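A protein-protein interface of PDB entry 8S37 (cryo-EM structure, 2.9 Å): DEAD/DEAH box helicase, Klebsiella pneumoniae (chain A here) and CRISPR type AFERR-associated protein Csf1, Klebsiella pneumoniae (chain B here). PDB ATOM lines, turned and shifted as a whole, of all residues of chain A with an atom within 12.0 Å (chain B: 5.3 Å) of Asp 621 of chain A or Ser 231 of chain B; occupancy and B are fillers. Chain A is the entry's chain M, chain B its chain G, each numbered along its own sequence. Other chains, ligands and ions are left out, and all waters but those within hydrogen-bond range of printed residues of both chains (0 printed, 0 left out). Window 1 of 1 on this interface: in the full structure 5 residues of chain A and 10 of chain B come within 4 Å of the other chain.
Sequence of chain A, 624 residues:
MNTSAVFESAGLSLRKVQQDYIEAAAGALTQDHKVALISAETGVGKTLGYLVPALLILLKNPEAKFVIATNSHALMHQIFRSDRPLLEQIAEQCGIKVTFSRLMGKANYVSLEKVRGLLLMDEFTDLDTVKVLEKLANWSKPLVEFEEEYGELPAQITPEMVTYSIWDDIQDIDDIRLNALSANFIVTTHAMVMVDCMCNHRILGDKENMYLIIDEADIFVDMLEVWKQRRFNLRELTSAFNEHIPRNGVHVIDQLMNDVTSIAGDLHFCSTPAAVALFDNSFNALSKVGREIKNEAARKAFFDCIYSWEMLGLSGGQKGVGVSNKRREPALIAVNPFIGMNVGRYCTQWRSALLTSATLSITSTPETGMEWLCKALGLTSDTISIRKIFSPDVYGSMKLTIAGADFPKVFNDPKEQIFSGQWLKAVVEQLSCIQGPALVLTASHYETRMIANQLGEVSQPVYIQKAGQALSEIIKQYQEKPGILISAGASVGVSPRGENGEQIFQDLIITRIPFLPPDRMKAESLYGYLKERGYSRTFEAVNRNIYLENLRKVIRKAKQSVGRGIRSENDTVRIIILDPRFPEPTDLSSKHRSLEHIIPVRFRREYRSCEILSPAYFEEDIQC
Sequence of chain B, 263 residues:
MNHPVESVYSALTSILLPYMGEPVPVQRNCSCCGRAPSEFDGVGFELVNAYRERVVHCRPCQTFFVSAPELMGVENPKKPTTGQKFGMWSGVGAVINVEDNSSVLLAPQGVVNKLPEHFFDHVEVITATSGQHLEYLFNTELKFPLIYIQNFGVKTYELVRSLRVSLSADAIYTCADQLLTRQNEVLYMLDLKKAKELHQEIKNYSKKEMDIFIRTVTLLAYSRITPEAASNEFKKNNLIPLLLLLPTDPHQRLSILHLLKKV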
ATOM      1  N   THR A 586     -17.710  42.938  -5.637  1.00  0.00           N
ATOM      2  CA  THR A 586     -18.058  41.543  -5.866  1.00  0.00           C
ATOM      3  C   THR A 586     -17.993  40.704  -4.599  1.00  0.00           C
ATOM      4  O   THR A 586     -18.617  39.639  -4.545  1.00  0.00           O
ATOM      5  CB  THR A 586     -17.127  40.934  -6.917  1.00  0.00           C
ATOM      6  OG1 THR A 586     -15.779  40.940  -6.429  1.00  0.00           O
ATOM      7  CG2 THR A 586     -17.195  41.725  -8.215  1.00  0.00           C
ATOM      8  N   ALA A 616      -8.421  41.302  -7.452  1.00  0.00           N
ATOM      9  CA  ALA A 616      -8.012  39.931  -7.198  1.00  0.00           C
ATOM     10  C   ALA A 616      -8.540  39.046  -8.313  1.00  0.00           C
ATOM     11  O   ALA A 616      -9.696  39.178  -8.728  1.00  0.00           O
ATOM     12  CB  ALA A 616      -8.530  39.438  -5.845  1.00  0.00           C
ATOM     13  N   TYR A 617      -7.661  38.170  -8.802  1.00  0.00           N
ATOM     14  CA  TYR A 617      -7.905  37.379 -10.004  1.00  0.00           C
ATOM     15  C   TYR A 617      -9.282  36.730  -9.998  1.00  0.00           C
ATOM     16  O   TYR A 617      -9.628  35.975  -9.084  1.00  0.00           O
ATOM     17  CB  TYR A 617      -6.813  36.313 -10.149  1.00  0.00           C
ATOM     18  CG  TYR A 617      -6.727  35.330  -9.001  1.00  0.00           C
ATOM     19  CD1 TYR A 617      -6.022  35.636  -7.845  1.00  0.00           C
ATOM     20  CD2 TYR A 617      -7.341  34.086  -9.081  1.00  0.00           C
ATOM     21  CE1 TYR A 617      -5.942  34.741  -6.797  1.00  0.00           C
ATOM     22  CE2 TYR A 617      -7.265  33.184  -8.039  1.00  0.00           C
ATOM     23  CZ  TYR A 617      -6.564  33.515  -6.900  1.00  0.00           C
ATOM     24  OH  TYR A 617      -6.484  32.618  -5.859  1.00  0.00           O
ATOM     25  N   PHE A 618     -10.074  37.062 -11.009  1.00  0.00           N
ATOM     26  CA  PHE A 618     -11.295  36.353 -11.341  1.00  0.00           C
ATOM     27  C   PHE A 618     -11.002  35.436 -12.522  1.00  0.00           C
ATOM     28  O   PHE A 618      -9.863  35.332 -12.986  1.00  0.00           O
ATOM     29  CB  PHE A 618     -12.428  37.339 -11.641  1.00  0.00           C
ATOM     30  CG  PHE A 618     -12.773  38.258 -10.495  1.00  0.00           C
ATOM     31  CD1 PHE A 618     -12.467  37.928  -9.182  1.00  0.00           C
ATOM     32  CD2 PHE A 618     -13.422  39.457 -10.739  1.00  0.00           C
ATOM     33  CE1 PHE A 618     -12.793  38.778  -8.144  1.00  0.00           C
ATOM     34  CE2 PHE A 618     -13.750  40.309  -9.704  1.00  0.00           C
ATOM     35  CZ  PHE A 618     -13.435  39.968  -8.405  1.00  0.00           C
ATOM     36  N   GLU A 619     -12.036  34.780 -13.035  1.00  0.00           N
ATOM     37  CA  GLU A 619     -11.880  33.816 -14.116  1.00  0.00           C
ATOM     38  C   GLU A 619     -13.219  33.705 -14.841  1.00  0.00           C
ATOM     39  O   GLU A 619     -14.135  34.503 -14.617  1.00  0.00           O
ATOM     40  CB  GLU A 619     -11.397  32.461 -13.577  1.00  0.00           C
ATOM     41  CG  GLU A 619      -9.967  32.448 -13.058  1.00  0.00           C
ATOM     42  CD  GLU A 619      -9.425  31.045 -12.868  1.00  0.00           C
ATOM     43  OE1 GLU A 619     -10.195  30.075 -13.033  1.00  0.00           O
ATOM     44  OE2 GLU A 619      -8.225  30.910 -12.554  1.00  0.00           O
ATOM     45  N   GLU A 620     -13.327  32.708 -15.713  1.00  0.00           N
ATOM     46  CA  GLU A 620     -14.486  32.467 -16.563  1.00  0.00           C
ATOM     47  C   GLU A 620     -15.117  31.126 -16.214  1.00  0.00           C
ATOM     48  O   GLU A 620     -15.625  30.415 -17.082  1.00  0.00           O
ATOM     49  CB  GLU A 620     -14.104  32.536 -18.044  1.00  0.00           C
ATOM     50  CG  GLU A 620     -12.932  31.641 -18.486  1.00  0.00           C
ATOM     51  CD  GLU A 620     -13.347  30.219 -18.817  1.00  0.00           C
ATOM     52  OE1 GLU A 620     -14.405  30.036 -19.454  1.00  0.00           O
ATOM     53  OE2 GLU A 620     -12.614  29.282 -18.435  1.00  0.00           O
ATOM     54  N   ASP A 621     -15.092  30.790 -14.919  1.00  0.00           N
ATOM     55  CA  ASP A 621     -15.329  29.433 -14.435  1.00  0.00           C
ATOM     56  C   ASP A 621     -16.576  28.823 -15.052  1.00  0.00           C
ATOM     57  O   ASP A 621     -17.683  29.341 -14.888  1.00  0.00           O
ATOM     58  CB  ASP A 621     -15.461  29.453 -12.911  1.00  0.00           C
ATOM     59  CG  ASP A 621     -14.212  29.958 -12.223  1.00  0.00           C
ATOM     60  OD1 ASP A 621     -13.112  29.793 -12.789  1.00  0.00           O
ATOM     61  OD2 ASP A 621     -14.332  30.520 -11.116  1.00  0.00           O
ATOM     62  N   ILE A 622     -16.370  27.720 -15.776  1.00  0.00           N
ATOM     63  CA  ILE A 622     -17.433  27.096 -16.557  1.00  0.00           C
ATOM     64  C   ILE A 622     -18.642  26.764 -15.696  1.00  0.00           C
ATOM     65  O   ILE A 622     -19.777  26.751 -16.187  1.00  0.00           O
ATOM     66  CB  ILE A 622     -16.881  25.842 -17.262  1.00  0.00           C
ATOM     67  CG1 ILE A 622     -17.805  25.419 -18.405  1.00  0.00           C
ATOM     68  CG2 ILE A 622     -16.687  24.709 -16.262  1.00  0.00           C
ATOM     69  CD1 ILE A 622     -17.663  26.278 -19.645  1.00  0.00           C
ATOM     70  N   GLN A 623     -18.430  26.495 -14.409  1.00  0.00           N
ATOM     71  CA  GLN A 623     -19.517  26.148 -13.496  1.00  0.00           C
ATOM     72  C   GLN A 623     -20.203  27.414 -12.973  1.00  0.00           C
ATOM     73  O   GLN A 623     -20.296  27.663 -11.773  1.00  0.00           O
ATOM     74  CB  GLN A 623     -18.988  25.283 -12.358  1.00  0.00           C
ATOM     75  CG  GLN A 623     -20.074  24.530 -11.594  1.00  0.00           C
ATOM     76  CD  GLN A 623     -20.490  25.208 -10.299  1.00  0.00           C
ATOM     77  OE1 GLN A 623     -19.683  25.855  -9.632  1.00  0.00           O
ATOM     78  NE2 GLN A 623     -21.759  25.063  -9.942  1.00  0.00           N
ATOM     79  N   CYS A 624     -20.659  28.240 -13.909  1.00  0.00           N
ATOM     80  CA  CYS A 624     -21.340  29.482 -13.570  1.00  0.00           C
ATOM     81  C   CYS A 624     -22.818  29.223 -13.308  1.00  0.00           C
ATOM     82  O   CYS A 624     -23.197  28.146 -12.851  1.00  0.00           O
ATOM     83  CB  CYS A 624     -21.175  30.509 -14.690  1.00  0.00           C
ATOM     84  SG  CYS A 624     -21.918  32.119 -14.335  1.00  0.00           S
ATOM     85  N   THR B 226     -13.809  24.254  -3.852  1.00  0.00           N
ATOM     86  CA  THR B 226     -14.326  25.534  -4.296  1.00  0.00           C
ATOM     87  C   THR B 226     -14.656  25.477  -5.788  1.00  0.00           C
ATOM     88  O   THR B 226     -14.043  24.710  -6.535  1.00  0.00           O
ATOM     89  CB  THR B 226     -13.310  26.643  -4.042  1.00  0.00           C
ATOM     90  OG1 THR B 226     -12.162  26.442  -4.876  1.00  0.00           O
ATOM     91  CG2 THR B 226     -12.879  26.655  -2.583  1.00  0.00           C
ATOM     92  N   PRO B 227     -15.631  26.268  -6.249  1.00  0.00           N
ATOM     93  CA  PRO B 227     -15.887  26.320  -7.697  1.00  0.00           C
ATOM     94  C   PRO B 227     -14.674  26.718  -8.507  1.00  0.00           C
ATOM     95  O   PRO B 227     -14.528  26.259  -9.644  1.00  0.00           O
ATOM     96  CB  PRO B 227     -17.005  27.360  -7.811  1.00  0.00           C
ATOM     97  CG  PRO B 227     -17.728  27.229  -6.552  1.00  0.00           C
ATOM     98  CD  PRO B 227     -16.677  26.993  -5.507  1.00  0.00           C
ATOM     99  N   GLU B 228     -13.801  27.568  -7.968  1.00  0.00           N
ATOM    100  CA  GLU B 228     -12.610  27.946  -8.718  1.00  0.00           C
ATOM    101  C   GLU B 228     -11.680  26.754  -8.896  1.00  0.00           C
ATOM    102  O   GLU B 228     -11.118  26.554  -9.980  1.00  0.00           O
ATOM    103  CB  GLU B 228     -11.901  29.098  -7.999  1.00  0.00           C
ATOM    104  CG  GLU B 228     -10.456  29.359  -8.417  1.00  0.00           C
ATOM    105  CD  GLU B 228     -10.297  29.570  -9.907  1.00  0.00           C
ATOM    106  OE1 GLU B 228     -11.302  29.876 -10.582  1.00  0.00           O
ATOM    107  OE2 GLU B 228      -9.160  29.431 -10.404  1.00  0.00           O
ATOM    108  N   ALA B 229     -11.544  25.923  -7.861  1.00  0.00           N
ATOM    109  CA  ALA B 229     -10.727  24.723  -7.995  1.00  0.00           C
ATOM    110  C   ALA B 229     -11.333  23.760  -9.006  1.00  0.00           C
ATOM    111  O   ALA B 229     -10.613  23.182  -9.831  1.00  0.00           O
ATOM    112  CB  ALA B 229     -10.569  24.043  -6.636  1.00  0.00           C
ATOM    113  N   ALA B 230     -12.653  23.571  -8.956  1.00  0.00           N
ATOM    114  CA  ALA B 230     -13.304  22.679  -9.909  1.00  0.00           C
ATOM    115  C   ALA B 230     -13.156  23.189 -11.335  1.00  0.00           C
ATOM    116  O   ALA B 230     -12.922  22.404 -12.259  1.00  0.00           O
ATOM    117  CB  ALA B 230     -14.780  22.518  -9.551  1.00  0.00           C
ATOM    118  N   SER B 231     -13.300  24.499 -11.537  1.00  0.00           N
ATOM    119  CA  SER B 231     -13.150  25.057 -12.875  1.00  0.00           C
ATOM    120  C   SER B 231     -11.724  24.889 -13.376  1.00  0.00           C
ATOM    121  O   SER B 231     -11.508  24.560 -14.548  1.00  0.00           O
ATOM    122  CB  SER B 231     -13.552  26.530 -12.876  1.00  0.00           C
ATOM    123  OG  SER B 231     -12.663  27.300 -12.090  1.00  0.00           O
ATOM    124  N   ASN B 232     -10.739  25.107 -12.503  1.00  0.00           N
ATOM    125  CA  ASN B 232      -9.352  24.862 -12.877  1.00  0.00           C
ATOM    126  C   ASN B 232      -9.153  23.411 -13.288  1.00  0.00           C
ATOM    127  O   ASN B 232      -8.515  23.122 -14.307  1.00  0.00           O
ATOM    128  CB  ASN B 232      -8.422  25.229 -11.723  1.00  0.00           C
ATOM    129  CG  ASN B 232      -8.430  26.712 -11.423  1.00  0.00           C
ATOM    130  OD1 ASN B 232      -8.786  27.524 -12.275  1.00  0.00           O
ATOM    131  ND2 ASN B 232      -8.033  27.074 -10.210  1.00  0.00           N
ATOM    132  N   GLU B 233      -9.678  22.480 -12.490  1.00  0.00           N
ATOM    133  CA  GLU B 233      -9.505  21.064 -12.794  1.00  0.00           C
ATOM    134  C   GLU B 233     -10.166  20.696 -14.119  1.00  0.00           C
ATOM    135  O   GLU B 233      -9.587  19.959 -14.925  1.00  0.00           O
ATOM    136  CB  GLU B 233     -10.069  20.221 -11.651  1.00  0.00           C
ATOM    137  CG  GLU B 233      -9.623  18.765 -11.660  1.00  0.00           C
ATOM    138  CD  GLU B 233     -10.447  17.910 -12.601  1.00  0.00           C
ATOM    139  OE1 GLU B 233     -11.691  17.953 -12.512  1.00  0.00           O
ATOM    140  OE2 GLU B 233      -9.848  17.200 -13.435  1.00  0.00           O
ATOM    141  N   PHE B 234     -11.378  21.199 -14.363  1.00  0.00           N
ATOM    142  CA  PHE B 234     -12.061  20.918 -15.623  1.00  0.00           C
ATOM    143  C   PHE B 234     -11.290  21.484 -16.808  1.00  0.00           C
ATOM    144  O   PHE B 234     -11.130  20.809 -17.833  1.00  0.00           O
ATOM    145  CB  PHE B 234     -13.485  21.480 -15.595  1.00  0.00           C
ATOM    146  CG  PHE B 234     -14.393  20.812 -14.593  1.00  0.00           C
ATOM    147  CD1 PHE B 234     -14.364  19.439 -14.404  1.00  0.00           C
ATOM    148  CD2 PHE B 234     -15.284  21.560 -13.844  1.00  0.00           C
ATOM    149  CE1 PHE B 234     -15.194  18.832 -13.488  1.00  0.00           C
ATOM    150  CE2 PHE B 234     -16.117  20.954 -12.924  1.00  0.00           C
ATOM    151  CZ  PHE B 234     -16.073  19.589 -12.747  1.00  0.00           C
ATOM    152  N   LYS B 235     -10.812  22.723 -16.694  1.00  0.00           N
ATOM    153  CA  LYS B 235     -10.072  23.330 -17.795  1.00  0.00           C
ATOM    154  C   LYS B 235      -8.773  22.582 -18.056  1.00  0.00           C
ATOM    155  O   LYS B 235      -8.390  22.372 -19.213  1.00  0.00           O
ATOM    156  CB  LYS B 235      -9.793  24.800 -17.486  1.00  0.00           C
ATOM    157  CG  LYS B 235     -11.039  25.671 -17.463  1.00  0.00           C
ATOM    158  CD  LYS B 235     -10.834  26.942 -16.646  1.00  0.00           C
ATOM    159  CE  LYS B 235      -9.687  27.800 -17.167  1.00  0.00           C
ATOM    160  NZ  LYS B 235      -9.836  28.145 -18.607  1.00  0.00           N
ATOM    161  N   LYS B 236      -8.082  22.172 -16.994  1.00  0.00           N
ATOM    162  CA  LYS B 236      -6.807  21.487 -17.162  1.00  0.00           C
ATOM    163  C   LYS B 236      -6.991  20.104 -17.774  1.00  0.00           C
ATOM    164  O   LYS B 236      -6.109  19.630 -18.498  1.00  0.00           O
ATOM    165  CB  LYS B 236      -6.105  21.376 -15.808  1.00  0.00           C
ATOM    166  CG  LYS B 236      -4.651  20.930 -15.875  1.00  0.00           C
ATOM    167  CD  LYS B 236      -4.118  20.532 -14.501  1.00  0.00           C
ATOM    168  CE  LYS B 236      -4.183  21.676 -13.496  1.00  0.00           C
ATOM    169  NZ  LYS B 236      -3.527  21.320 -12.208  1.00  0.00           N
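Tyr 617 of chain A touches none of the printed residues of chain B.
Printed residues of chain B within 4 Å of Glu 619 of chain A: Glu 228 (2.7 Å), Ser 231 (3.8 Å) and Asn 232 (3.0 Å).
Printed residues of chain B within 4 Å of Glu 620 of chain A: Lys 235 (3.0 Å).
Of chain B, only Glu 228 and Ser 231 come within 4 Å of Asp 621 of chain A.
Of the printed residues of chain B, Gln 623 of chain A touches Pro 227 (3.6 Å).
Pro 227 of chain B touches one residue of chain A.
Glu 228 of chain B touches just these residues of chain A: Glu 619 and Asp 621.
No residue of chain A comes within 4 Å of Ala 229 of chain B.
No residue of chain A comes within 4 Å of Ala 230 of chain B.
Ser 231 of chain B touches two residues of chain A.
Lys 235 of chain B touches just one residue of chain A: Glu 620 (3.0 Å).
The nearest residue of chain A that does not touch Ser 231 of chain B is Ile 622 of chain A (4.2 Å).
OE2 of Glu 228 of chain B sits at hydrogen-bond distance from ND2 of Asn 232 of chain B.
O of Pro 227 of chain B sits at hydrogen-bond distance from OG of Ser 231 of chain B.
The backbone carbonyl oxygen (O) of Glu 228 of chain B sits at hydrogen-bond distance from the side-chain hydroxyl (OG) of Ser 231 of chain B (2.7 Å).
Among the printed residues, pairs that only touch across the chains: Gln 623 of chain A with Pro 227 of chain B (3.6 Å) and Glu 619 of chain A with Ser 231 of chain B (3.8 Å).
Hydrophobic or aromatic side chains of chain B within 4 Å of the printed part of chain A: Pro 227.
Printed residues of chain A that touch a printed residue of chain B: Glu 619, Glu 620, Asp 621 and Gln 623.
Among the printed residues, 7 pairs touch across the chains.
Among the printed residues, Asp or Glu carboxylates within 4 Å of a Lys or Arg side-chain nitrogen of the other chain: Glu 620 of chain A with Lys 235 of chain B (3.0 Å).
The side-chain carboxylate of Asp 621 of chain A lies within hydrogen-bond range of the side-chain hydroxyl of Ser 231 of chain B (2.6 Å).
The side-chain carboxylate (OE1) of Glu 619 of chain A lies close to the side-chain amide oxygen (OD1) of Asn 232 of chain B (3.0 Å).
OD1 of Asp 621 of chain A sits close to OE1 of Glu 228 of chain B, 2.9 Å away.
The side-chain carboxylate of Glu 620 of chain A is in salt-bridge range of the side-chain amino group of Lys 235 of chain B, 3.0 Å away.
OE1 of Glu 228 of chain B sits close to OE1 of Glu 619 of chain A (2.7 Å).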
